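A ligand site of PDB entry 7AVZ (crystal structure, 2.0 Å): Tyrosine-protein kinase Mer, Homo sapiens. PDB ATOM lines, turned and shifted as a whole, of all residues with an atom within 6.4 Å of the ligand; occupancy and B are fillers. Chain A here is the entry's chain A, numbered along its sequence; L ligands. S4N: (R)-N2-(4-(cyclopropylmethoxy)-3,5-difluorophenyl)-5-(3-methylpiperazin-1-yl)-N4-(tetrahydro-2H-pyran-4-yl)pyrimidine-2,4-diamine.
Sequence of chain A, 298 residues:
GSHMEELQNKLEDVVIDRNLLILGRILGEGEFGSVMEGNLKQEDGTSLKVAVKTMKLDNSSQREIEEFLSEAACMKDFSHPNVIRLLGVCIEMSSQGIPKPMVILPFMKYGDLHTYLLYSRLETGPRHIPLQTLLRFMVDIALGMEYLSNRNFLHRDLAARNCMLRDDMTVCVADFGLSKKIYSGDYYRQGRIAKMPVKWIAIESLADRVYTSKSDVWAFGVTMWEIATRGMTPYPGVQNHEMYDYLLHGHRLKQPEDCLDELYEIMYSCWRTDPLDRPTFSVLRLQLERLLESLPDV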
ATOM      1  N   LEU A  27       8.160 -36.183 -22.974  1.00  0.00           N
ATOM      2  CA  LEU A  27       7.983 -34.751 -23.258  1.00  0.00           C
ATOM      3  C   LEU A  27       8.842 -34.284 -24.451  1.00  0.00           C
ATOM      4  O   LEU A  27       8.525 -33.280 -25.074  1.00  0.00           O
ATOM      5  CB  LEU A  27       8.308 -33.907 -22.005  1.00  0.00           C
ATOM      6  CG  LEU A  27       7.540 -34.217 -20.711  1.00  0.00           C
ATOM      7  CD1 LEU A  27       8.123 -33.457 -19.535  1.00  0.00           C
ATOM      8  CD2 LEU A  27       6.044 -33.926 -20.850  1.00  0.00           C
ATOM      9  N   GLY A  28       9.925 -35.004 -24.725  1.00  0.00           N
ATOM     10  CA  GLY A  28      10.857 -34.720 -25.805  1.00  0.00           C
ATOM     11  C   GLY A  28      11.876 -35.821 -26.014  1.00  0.00           C
ATOM     12  O   GLY A  28      12.221 -36.516 -25.057  1.00  0.00           O
ATOM     13  N   VAL A  35      13.450 -36.694 -22.532  1.00  0.00           N
ATOM     14  CA  VAL A  35      12.883 -36.003 -21.369  1.00  0.00           C
ATOM     15  C   VAL A  35      11.501 -36.600 -21.130  1.00  0.00           C
ATOM     16  O   VAL A  35      10.708 -36.714 -22.065  1.00  0.00           O
ATOM     17  CB  VAL A  35      12.904 -34.458 -21.481  1.00  0.00           C
ATOM     18  CG1 VAL A  35      12.395 -33.805 -20.191  1.00  0.00           C
ATOM     19  CG2 VAL A  35      14.315 -33.947 -21.796  1.00  0.00           C
ATOM     20  N   GLU A  37       8.073 -36.938 -18.189  1.00  0.00           N
ATOM     21  CA  GLU A  37       7.438 -36.405 -16.995  1.00  0.00           C
ATOM     22  C   GLU A  37       7.529 -37.524 -15.949  1.00  0.00           C
ATOM     23  O   GLU A  37       7.603 -38.698 -16.327  1.00  0.00           O
ATOM     24  CB  GLU A  37       5.988 -35.959 -17.267  1.00  0.00           C
ATOM     25  CG  GLU A  37       5.119 -36.991 -17.977  1.00  0.00           C
ATOM     26  CD  GLU A  37       3.948 -37.534 -17.189  1.00  0.00           C
ATOM     27  OE1 GLU A  37       3.409 -36.795 -16.336  1.00  0.00           O
ATOM     28  OE2 GLU A  37       3.549 -38.701 -17.438  1.00  0.00           O
ATOM     29  N   VAL A  50       8.028 -34.162 -11.351  1.00  0.00           N
ATOM     30  CA  VAL A  50       9.386 -33.879 -11.828  1.00  0.00           C
ATOM     31  C   VAL A  50       9.501 -34.134 -13.336  1.00  0.00           C
ATOM     32  O   VAL A  50       8.589 -34.682 -13.946  1.00  0.00           O
ATOM     33  CB  VAL A  50      10.454 -34.713 -11.050  1.00  0.00           C
ATOM     34  CG1 VAL A  50      10.517 -34.327  -9.571  1.00  0.00           C
ATOM     35  CG2 VAL A  50      10.233 -36.229 -11.222  1.00  0.00           C
ATOM     36  N   ALA A  51      10.646 -33.748 -13.915  1.00  0.00           N
ATOM     37  CA  ALA A  51      11.033 -34.011 -15.300  1.00  0.00           C
ATOM     38  C   ALA A  51      12.292 -34.870 -15.191  1.00  0.00           C
ATOM     39  O   ALA A  51      13.160 -34.575 -14.374  1.00  0.00           O
ATOM     40  CB  ALA A  51      11.334 -32.712 -16.020  1.00  0.00           C
ATOM     41  N   VAL A  52      12.374 -35.943 -15.963  1.00  0.00           N
ATOM     42  CA  VAL A  52      13.509 -36.861 -15.950  1.00  0.00           C
ATOM     43  C   VAL A  52      14.181 -36.824 -17.321  1.00  0.00           C
ATOM     44  O   VAL A  52      13.531 -37.119 -18.334  1.00  0.00           O
ATOM     45  CB  VAL A  52      13.139 -38.300 -15.514  1.00  0.00           C
ATOM     46  CG1 VAL A  52      14.380 -39.189 -15.375  1.00  0.00           C
ATOM     47  CG2 VAL A  52      12.347 -38.314 -14.210  1.00  0.00           C
ATOM     48  N   LYS A  53      15.473 -36.461 -17.355  1.00  0.00           N
ATOM     49  CA  LYS A  53      16.276 -36.400 -18.566  1.00  0.00           C
ATOM     50  C   LYS A  53      17.199 -37.612 -18.541  1.00  0.00           C
ATOM     51  O   LYS A  53      17.986 -37.767 -17.611  1.00  0.00           O
ATOM     52  CB  LYS A  53      17.065 -35.074 -18.629  1.00  0.00           C
ATOM     53  CG  LYS A  53      17.857 -34.860 -19.909  1.00  0.00           C
ATOM     54  CD  LYS A  53      18.264 -33.397 -20.062  1.00  0.00           C
ATOM     55  CE  LYS A  53      19.017 -33.145 -21.358  1.00  0.00           C
ATOM     56  NZ  LYS A  53      20.415 -33.640 -21.294  1.00  0.00           N
ATOM     57  N   ILE A  84      18.720 -23.381 -12.534  1.00  0.00           N
ATOM     58  CA  ILE A  84      17.926 -24.603 -12.352  1.00  0.00           C
ATOM     59  C   ILE A  84      18.485 -25.445 -11.201  1.00  0.00           C
ATOM     60  O   ILE A  84      19.699 -25.629 -11.110  1.00  0.00           O
ATOM     61  CB  ILE A  84      17.723 -25.427 -13.671  1.00  0.00           C
ATOM     62  CG1 ILE A  84      16.520 -26.406 -13.537  1.00  0.00           C
ATOM     63  CG2 ILE A  84      18.963 -26.212 -14.076  1.00  0.00           C
ATOM     64  CD1 ILE A  84      15.242 -25.823 -13.988  1.00  0.00           C
ATOM     65  N   VAL A 103      18.733 -37.766 -14.934  1.00  0.00           N
ATOM     66  CA  VAL A 103      18.861 -36.556 -14.120  1.00  0.00           C
ATOM     67  C   VAL A 103      17.428 -36.092 -13.752  1.00  0.00           C
ATOM     68  O   VAL A 103      16.540 -36.067 -14.605  1.00  0.00           O
ATOM     69  CB  VAL A 103      19.821 -35.458 -14.688  1.00  0.00           C
ATOM     70  CG1 VAL A 103      20.751 -36.005 -15.779  1.00  0.00           C
ATOM     71  CG2 VAL A 103      19.096 -34.226 -15.173  1.00  0.00           C
ATOM     72  N   LEU A 105      14.851 -33.369 -12.478  1.00  0.00           N
ATOM     73  CA  LEU A 105      14.754 -31.920 -12.549  1.00  0.00           C
ATOM     74  C   LEU A 105      13.359 -31.395 -12.184  1.00  0.00           C
ATOM     75  O   LEU A 105      12.401 -32.163 -12.244  1.00  0.00           O
ATOM     76  CB  LEU A 105      15.102 -31.506 -14.005  1.00  0.00           C
ATOM     77  CG  LEU A 105      16.531 -31.747 -14.471  1.00  0.00           C
ATOM     78  CD1 LEU A 105      16.589 -31.941 -15.981  1.00  0.00           C
ATOM     79  CD2 LEU A 105      17.456 -30.616 -14.060  1.00  0.00           C
ATOM     80  N   PRO A 106      13.204 -30.095 -11.843  1.00  0.00           N
ATOM     81  CA  PRO A 106      11.866 -29.570 -11.533  1.00  0.00           C
ATOM     82  C   PRO A 106      10.931 -29.631 -12.745  1.00  0.00           C
ATOM     83  O   PRO A 106      11.385 -29.529 -13.889  1.00  0.00           O
ATOM     84  CB  PRO A 106      12.141 -28.103 -11.142  1.00  0.00           C
ATOM     85  CG  PRO A 106      13.589 -28.077 -10.766  1.00  0.00           C
ATOM     86  CD  PRO A 106      14.223 -29.023 -11.724  1.00  0.00           C
ATOM     87  N   PHE A 107       9.636 -29.813 -12.491  1.00  0.00           N
ATOM     88  CA  PHE A 107       8.632 -29.831 -13.551  1.00  0.00           C
ATOM     89  C   PHE A 107       8.181 -28.393 -13.723  1.00  0.00           C
ATOM     90  O   PHE A 107       7.721 -27.760 -12.762  1.00  0.00           O
ATOM     91  CB  PHE A 107       7.428 -30.736 -13.200  1.00  0.00           C
ATOM     92  CG  PHE A 107       6.433 -30.879 -14.322  1.00  0.00           C
ATOM     93  CD1 PHE A 107       6.586 -31.865 -15.286  1.00  0.00           C
ATOM     94  CD2 PHE A 107       5.353 -30.012 -14.438  1.00  0.00           C
ATOM     95  CE1 PHE A 107       5.685 -31.986 -16.341  1.00  0.00           C
ATOM     96  CE2 PHE A 107       4.447 -30.125 -15.490  1.00  0.00           C
ATOM     97  CZ  PHE A 107       4.600 -31.129 -16.429  1.00  0.00           C
ATOM     98  N   MET A 108       8.357 -27.850 -14.944  1.00  0.00           N
ATOM     99  CA  MET A 108       8.008 -26.466 -15.243  1.00  0.00           C
ATOM    100  C   MET A 108       7.085 -26.365 -16.441  1.00  0.00           C
ATOM    101  O   MET A 108       7.522 -26.417 -17.598  1.00  0.00           O
ATOM    102  CB  MET A 108       9.266 -25.616 -15.399  1.00  0.00           C
ATOM    103  CG  MET A 108      10.177 -25.735 -14.208  1.00  0.00           C
ATOM    104  SD  MET A 108      11.861 -25.439 -14.673  1.00  0.00           S
ATOM    105  CE  MET A 108      12.005 -23.827 -14.055  1.00  0.00           C
ATOM    106  N   LYS A 109       5.789 -26.227 -16.113  1.00  0.00           N
ATOM    107  CA  LYS A 109       4.667 -26.142 -17.043  1.00  0.00           C
ATOM    108  C   LYS A 109       4.889 -25.160 -18.205  1.00  0.00           C
ATOM    109  O   LYS A 109       4.443 -25.464 -19.300  1.00  0.00           O
ATOM    110  CB  LYS A 109       3.350 -25.818 -16.293  1.00  0.00           C
ATOM    111  CG  LYS A 109       3.330 -24.471 -15.547  1.00  0.00           C
ATOM    112  CD  LYS A 109       1.963 -24.170 -14.952  1.00  0.00           C
ATOM    113  CE  LYS A 109       1.926 -22.795 -14.329  1.00  0.00           C
ATOM    114  NZ  LYS A 109       0.631 -22.525 -13.656  1.00  0.00           N
ATOM    115  N   TYR A 110       5.610 -24.034 -17.984  1.00  0.00           N
ATOM    116  CA  TYR A 110       5.815 -23.066 -19.079  1.00  0.00           C
ATOM    117  C   TYR A 110       6.929 -23.460 -20.051  1.00  0.00           C
ATOM    118  O   TYR A 110       7.010 -22.863 -21.132  1.00  0.00           O
ATOM    119  CB  TYR A 110       6.002 -21.633 -18.565  1.00  0.00           C
ATOM    120  CG  TYR A 110       4.788 -21.053 -17.860  1.00  0.00           C
ATOM    121  CD1 TYR A 110       3.543 -21.040 -18.484  1.00  0.00           C
ATOM    122  CD2 TYR A 110       4.889 -20.515 -16.580  1.00  0.00           C
ATOM    123  CE1 TYR A 110       2.419 -20.524 -17.826  1.00  0.00           C
ATOM    124  CE2 TYR A 110       3.779 -19.976 -15.933  1.00  0.00           C
ATOM    125  CZ  TYR A 110       2.545 -19.979 -16.561  1.00  0.00           C
ATOM    126  OH  TYR A 110       1.463 -19.447 -15.911  1.00  0.00           O
ATOM    127  N   GLY A 111       7.733 -24.470 -19.692  1.00  0.00           N
ATOM    128  CA  GLY A 111       8.790 -25.009 -20.553  1.00  0.00           C
ATOM    129  C   GLY A 111       9.935 -24.048 -20.832  1.00  0.00           C
ATOM    130  O   GLY A 111      10.197 -23.136 -20.029  1.00  0.00           O
ATOM    131  N   ASP A 112      10.661 -24.289 -21.933  1.00  0.00           N
ATOM    132  CA  ASP A 112      11.833 -23.491 -22.326  1.00  0.00           C
ATOM    133  C   ASP A 112      11.450 -22.126 -22.862  1.00  0.00           C
ATOM    134  O   ASP A 112      10.389 -21.972 -23.480  1.00  0.00           O
ATOM    135  CB  ASP A 112      12.749 -24.240 -23.304  1.00  0.00           C
ATOM    136  CG  ASP A 112      12.213 -24.339 -24.722  1.00  0.00           C
ATOM    137  OD1 ASP A 112      11.395 -25.238 -24.992  1.00  0.00           O
ATOM    138  OD2 ASP A 112      12.626 -23.519 -25.570  1.00  0.00           O
ATOM    139  N   THR A 115      10.734 -21.687 -26.993  1.00  0.00           N
ATOM    140  CA  THR A 115       9.397 -22.128 -27.400  1.00  0.00           C
ATOM    141  C   THR A 115       8.346 -21.112 -26.947  1.00  0.00           C
ATOM    142  O   THR A 115       7.446 -20.775 -27.720  1.00  0.00           O
ATOM    143  CB  THR A 115       9.114 -23.543 -26.876  1.00  0.00           C
ATOM    144  OG1 THR A 115      10.211 -24.380 -27.240  1.00  0.00           O
ATOM    145  CG2 THR A 115       7.865 -24.140 -27.480  1.00  0.00           C
ATOM    146  N   ARG A 161      16.848 -21.653 -25.733  1.00  0.00           N
ATOM    147  CA  ARG A 161      16.327 -23.026 -25.667  1.00  0.00           C
ATOM    148  C   ARG A 161      16.747 -23.726 -24.356  1.00  0.00           C
ATOM    149  O   ARG A 161      16.065 -24.654 -23.915  1.00  0.00           O
ATOM    150  CB  ARG A 161      16.748 -23.852 -26.914  1.00  0.00           C
ATOM    151  CG  ARG A 161      18.238 -24.156 -26.962  1.00  0.00           C
ATOM    152  CD  ARG A 161      18.735 -24.819 -28.236  1.00  0.00           C
ATOM    153  NE  ARG A 161      20.192 -24.874 -28.249  1.00  0.00           N
ATOM    154  CZ  ARG A 161      20.975 -23.933 -28.785  1.00  0.00           C
ATOM    155  NH1 ARG A 161      20.443 -22.868 -29.375  1.00  0.00           N
ATOM    156  NH2 ARG A 161      22.296 -24.062 -28.742  1.00  0.00           N
ATOM    157  N   ASN A 162      17.869 -23.271 -23.748  1.00  0.00           N
ATOM    158  CA  ASN A 162      18.391 -23.832 -22.500  1.00  0.00           C
ATOM    159  C   ASN A 162      18.050 -22.985 -21.274  1.00  0.00           C
ATOM    160  O   ASN A 162      18.605 -23.221 -20.211  1.00  0.00           O
ATOM    161  CB  ASN A 162      19.893 -24.114 -22.613  1.00  0.00           C
ATOM    162  CG  ASN A 162      20.191 -25.159 -23.655  1.00  0.00           C
ATOM    163  OD1 ASN A 162      19.510 -26.183 -23.782  1.00  0.00           O
ATOM    164  ND2 ASN A 162      21.218 -24.911 -24.452  1.00  0.00           N
ATOM    165  N   CYS A 163      17.129 -22.027 -21.405  1.00  0.00           N
ATOM    166  CA  CYS A 163      16.637 -21.232 -20.279  1.00  0.00           C
ATOM    167  C   CYS A 163      15.216 -21.691 -20.012  1.00  0.00           C
ATOM    168  O   CYS A 163      14.466 -21.895 -20.959  1.00  0.00           O
ATOM    169  CB  CYS A 163      16.713 -19.743 -20.582  1.00  0.00           C
ATOM    170  SG  CYS A 163      18.391 -19.146 -20.840  1.00  0.00           S
ATOM    171  N   MET A 164      14.867 -21.923 -18.731  1.00  0.00           N
ATOM    172  CA  MET A 164      13.549 -22.432 -18.376  1.00  0.00           C
ATOM    173  C   MET A 164      12.696 -21.389 -17.684  1.00  0.00           C
ATOM    174  O   MET A 164      13.236 -20.490 -17.058  1.00  0.00           O
ATOM    175  CB  MET A 164      13.650 -23.720 -17.523  1.00  0.00           C
ATOM    176  CG  MET A 164      14.323 -24.897 -18.240  1.00  0.00           C
ATOM    177  SD  MET A 164      13.417 -25.608 -19.653  1.00  0.00           S
ATOM    178  CE  MET A 164      12.007 -26.347 -18.835  1.00  0.00           C
ATOM    179  N   ALA A 174      19.740 -23.228 -17.464  1.00  0.00           N
ATOM    180  CA  ALA A 174      19.760 -24.690 -17.392  1.00  0.00           C
ATOM    181  C   ALA A 174      20.670 -25.277 -18.467  1.00  0.00           C
ATOM    182  O   ALA A 174      21.220 -24.536 -19.273  1.00  0.00           O
ATOM    183  CB  ALA A 174      18.331 -25.221 -17.546  1.00  0.00           C
ATOM    184  N   ASP A 175      20.844 -26.628 -18.457  1.00  0.00           N
ATOM    185  CA  ASP A 175      21.617 -27.435 -19.416  1.00  0.00           C
ATOM    186  C   ASP A 175      23.066 -26.960 -19.619  1.00  0.00           C
ATOM    187  O   ASP A 175      23.547 -26.810 -20.743  1.00  0.00           O
ATOM    188  CB  ASP A 175      20.880 -27.547 -20.759  1.00  0.00           C
ATOM    189  CG  ASP A 175      21.172 -28.786 -21.589  1.00  0.00           C
ATOM    190  OD1 ASP A 175      22.083 -29.553 -21.203  1.00  0.00           O
ATOM    191  OD2 ASP A 175      20.508 -28.977 -22.622  1.00  0.00           O
HETATM  192  C1  S4N L   1       4.551 -30.143 -20.841  1.00  0.00           C
HETATM  193  C2  S4N L   1       5.767 -30.298 -19.863  1.00  0.00           C
HETATM  194  C3  S4N L   1       6.635 -28.131 -20.690  1.00  0.00           C
HETATM  195  C7  S4N L   1      10.234 -29.571 -17.747  1.00  0.00           C
HETATM  196  C8  S4N L   1       9.365 -29.609 -19.882  1.00  0.00           C
HETATM  197  C9  S4N L   1      10.903 -29.724 -21.795  1.00  0.00           C
HETATM  198  C10 S4N L   1      11.132 -31.034 -22.543  1.00  0.00           C
HETATM  199  C11 S4N L   1      12.496 -31.009 -23.201  1.00  0.00           C
HETATM  200  C12 S4N L   1      12.510 -28.654 -23.344  1.00  0.00           C
HETATM  201  C13 S4N L   1      11.143 -28.529 -22.712  1.00  0.00           C
HETATM  202  C14 S4N L   1      12.709 -29.606 -17.351  1.00  0.00           C
HETATM  203  C15 S4N L   1      13.133 -30.384 -18.419  1.00  0.00           C
HETATM  204  C16 S4N L   1      14.457 -30.352 -18.783  1.00  0.00           C
HETATM  205  C19 S4N L   1      13.621 -28.807 -16.667  1.00  0.00           C
HETATM  206  C20 S4N L   1      17.174 -28.398 -19.176  1.00  0.00           C
HETATM  207  C21 S4N L   1      16.569 -28.273 -20.553  1.00  0.00           C
HETATM  208  C22 S4N L   1      16.535 -26.936 -21.205  1.00  0.00           C
HETATM  209  F1  S4N L   1      14.860 -31.115 -19.818  1.00  0.00           F
HETATM  210  C17 S4N L   1      15.409 -29.581 -18.133  1.00  0.00           C
HETATM  211  O1  S4N L   1      16.722 -29.621 -18.587  1.00  0.00           O
HETATM  212  C23 S4N L   1      17.443 -27.992 -21.731  1.00  0.00           C
HETATM  213  C18 S4N L   1      14.931 -28.813 -17.067  1.00  0.00           C
HETATM  214  F   S4N L   1      15.810 -28.032 -16.396  1.00  0.00           F
HETATM  215  N5  S4N L   1      11.355 -29.602 -16.960  1.00  0.00           N
HETATM  216  N2  S4N L   1       9.055 -29.469 -17.130  1.00  0.00           N
HETATM  217  C6  S4N L   1       7.986 -29.438 -17.930  1.00  0.00           C
HETATM  218  N3  S4N L   1      10.432 -29.643 -19.073  1.00  0.00           N
HETATM  219  N4  S4N L   1       9.577 -29.685 -21.206  1.00  0.00           N
HETATM  220  O   S4N L   1      12.635 -29.878 -24.071  1.00  0.00           O
HETATM  221  C5  S4N L   1       8.051 -29.508 -19.322  1.00  0.00           C
HETATM  222  N   S4N L   1       6.931 -29.473 -20.184  1.00  0.00           N
HETATM  223  C4  S4N L   1       5.661 -28.179 -21.852  1.00  0.00           C
HETATM  224  N1  S4N L   1       4.382 -28.755 -21.405  1.00  0.00           N
HETATM  225  C   S4N L   1       3.243 -30.521 -20.162  1.00  0.00           C
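The backbone NH (N) of Met 108 sits at hydrogen-bond distance from a nitrogen (N2) of the ligand (2.8 Å).
O of Pro 106 sits at hydrogen-bond distance from N5 of the ligand, 3.1 Å away.
O of Asn 162 lies within hydrogen-bond range of N of Ala 174.
The side-chain carboxylate (OD1) of Asp 112 lies within hydrogen-bond range of the side-chain hydroxyl (OG1) of Thr 115 (2.7 Å).
The side-chain carboxylate (OD2) of Asp 175 lies close to the side-chain amide oxygen (OD1) of Asn 162 (3.2 Å).
O of Ala 51 lies within hydrogen-bond range of N of Leu 105, at 2.8 Å.
The backbone NH of Val 35 is in hydrogen-bond range of the backbone carbonyl oxygen of Gly 28 (2.8 Å).
The backbone NH (N) of Leu 27 is in hydrogen-bond range of the backbone carbonyl oxygen (O) of Val 35, 2.8 Å away.
Leu 27 touches the ligand.
Val 35 touches the ligand (CG2 to F1, 3.5 Å).
Ala 51 touches the ligand (CB to N5, 3.2 Å).
Ile 84 touches the ligand.
CD1 of Leu 105 touches C17 of the ligand (3.4 Å).
Phe 107 touches the ligand.
Lys 109 touches the ligand.
CA of Gly 111 touches C3 of the ligand (3.8 Å).
Asp 112 touches the ligand.
O of Arg 161 touches C22 of the ligand, at 3.6 Å.
OD1 of Asn 162 touches C23 of the ligand (3.4 Å).
CE of Met 164 touches C14 of the ligand, at 3.6 Å.
CB of Ala 174 touches C20 of the ligand (3.8 Å).
Asp 175 touches the ligand (OD2 to C23, 3.3 Å).
Hydrophobic or aromatic side chains within 4 Å of the ligand: Leu 27, Val 35, Ala 51, Ile 84, Leu 105, Phe 107, Met 164 and Ala 174.
Within 4 Å of the ligand: Leu 27, Val 35, Ala 51, Ile 84, Leu 105, Pro 106, Phe 107, Met 108, Lys 109, Gly 111, Asp 112, Arg 161, Asn 162, Met 164, Ala 174 and Asp 175.
The nearest printed residue that does not touch the ligand is Lys 53 (4.1 Å).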
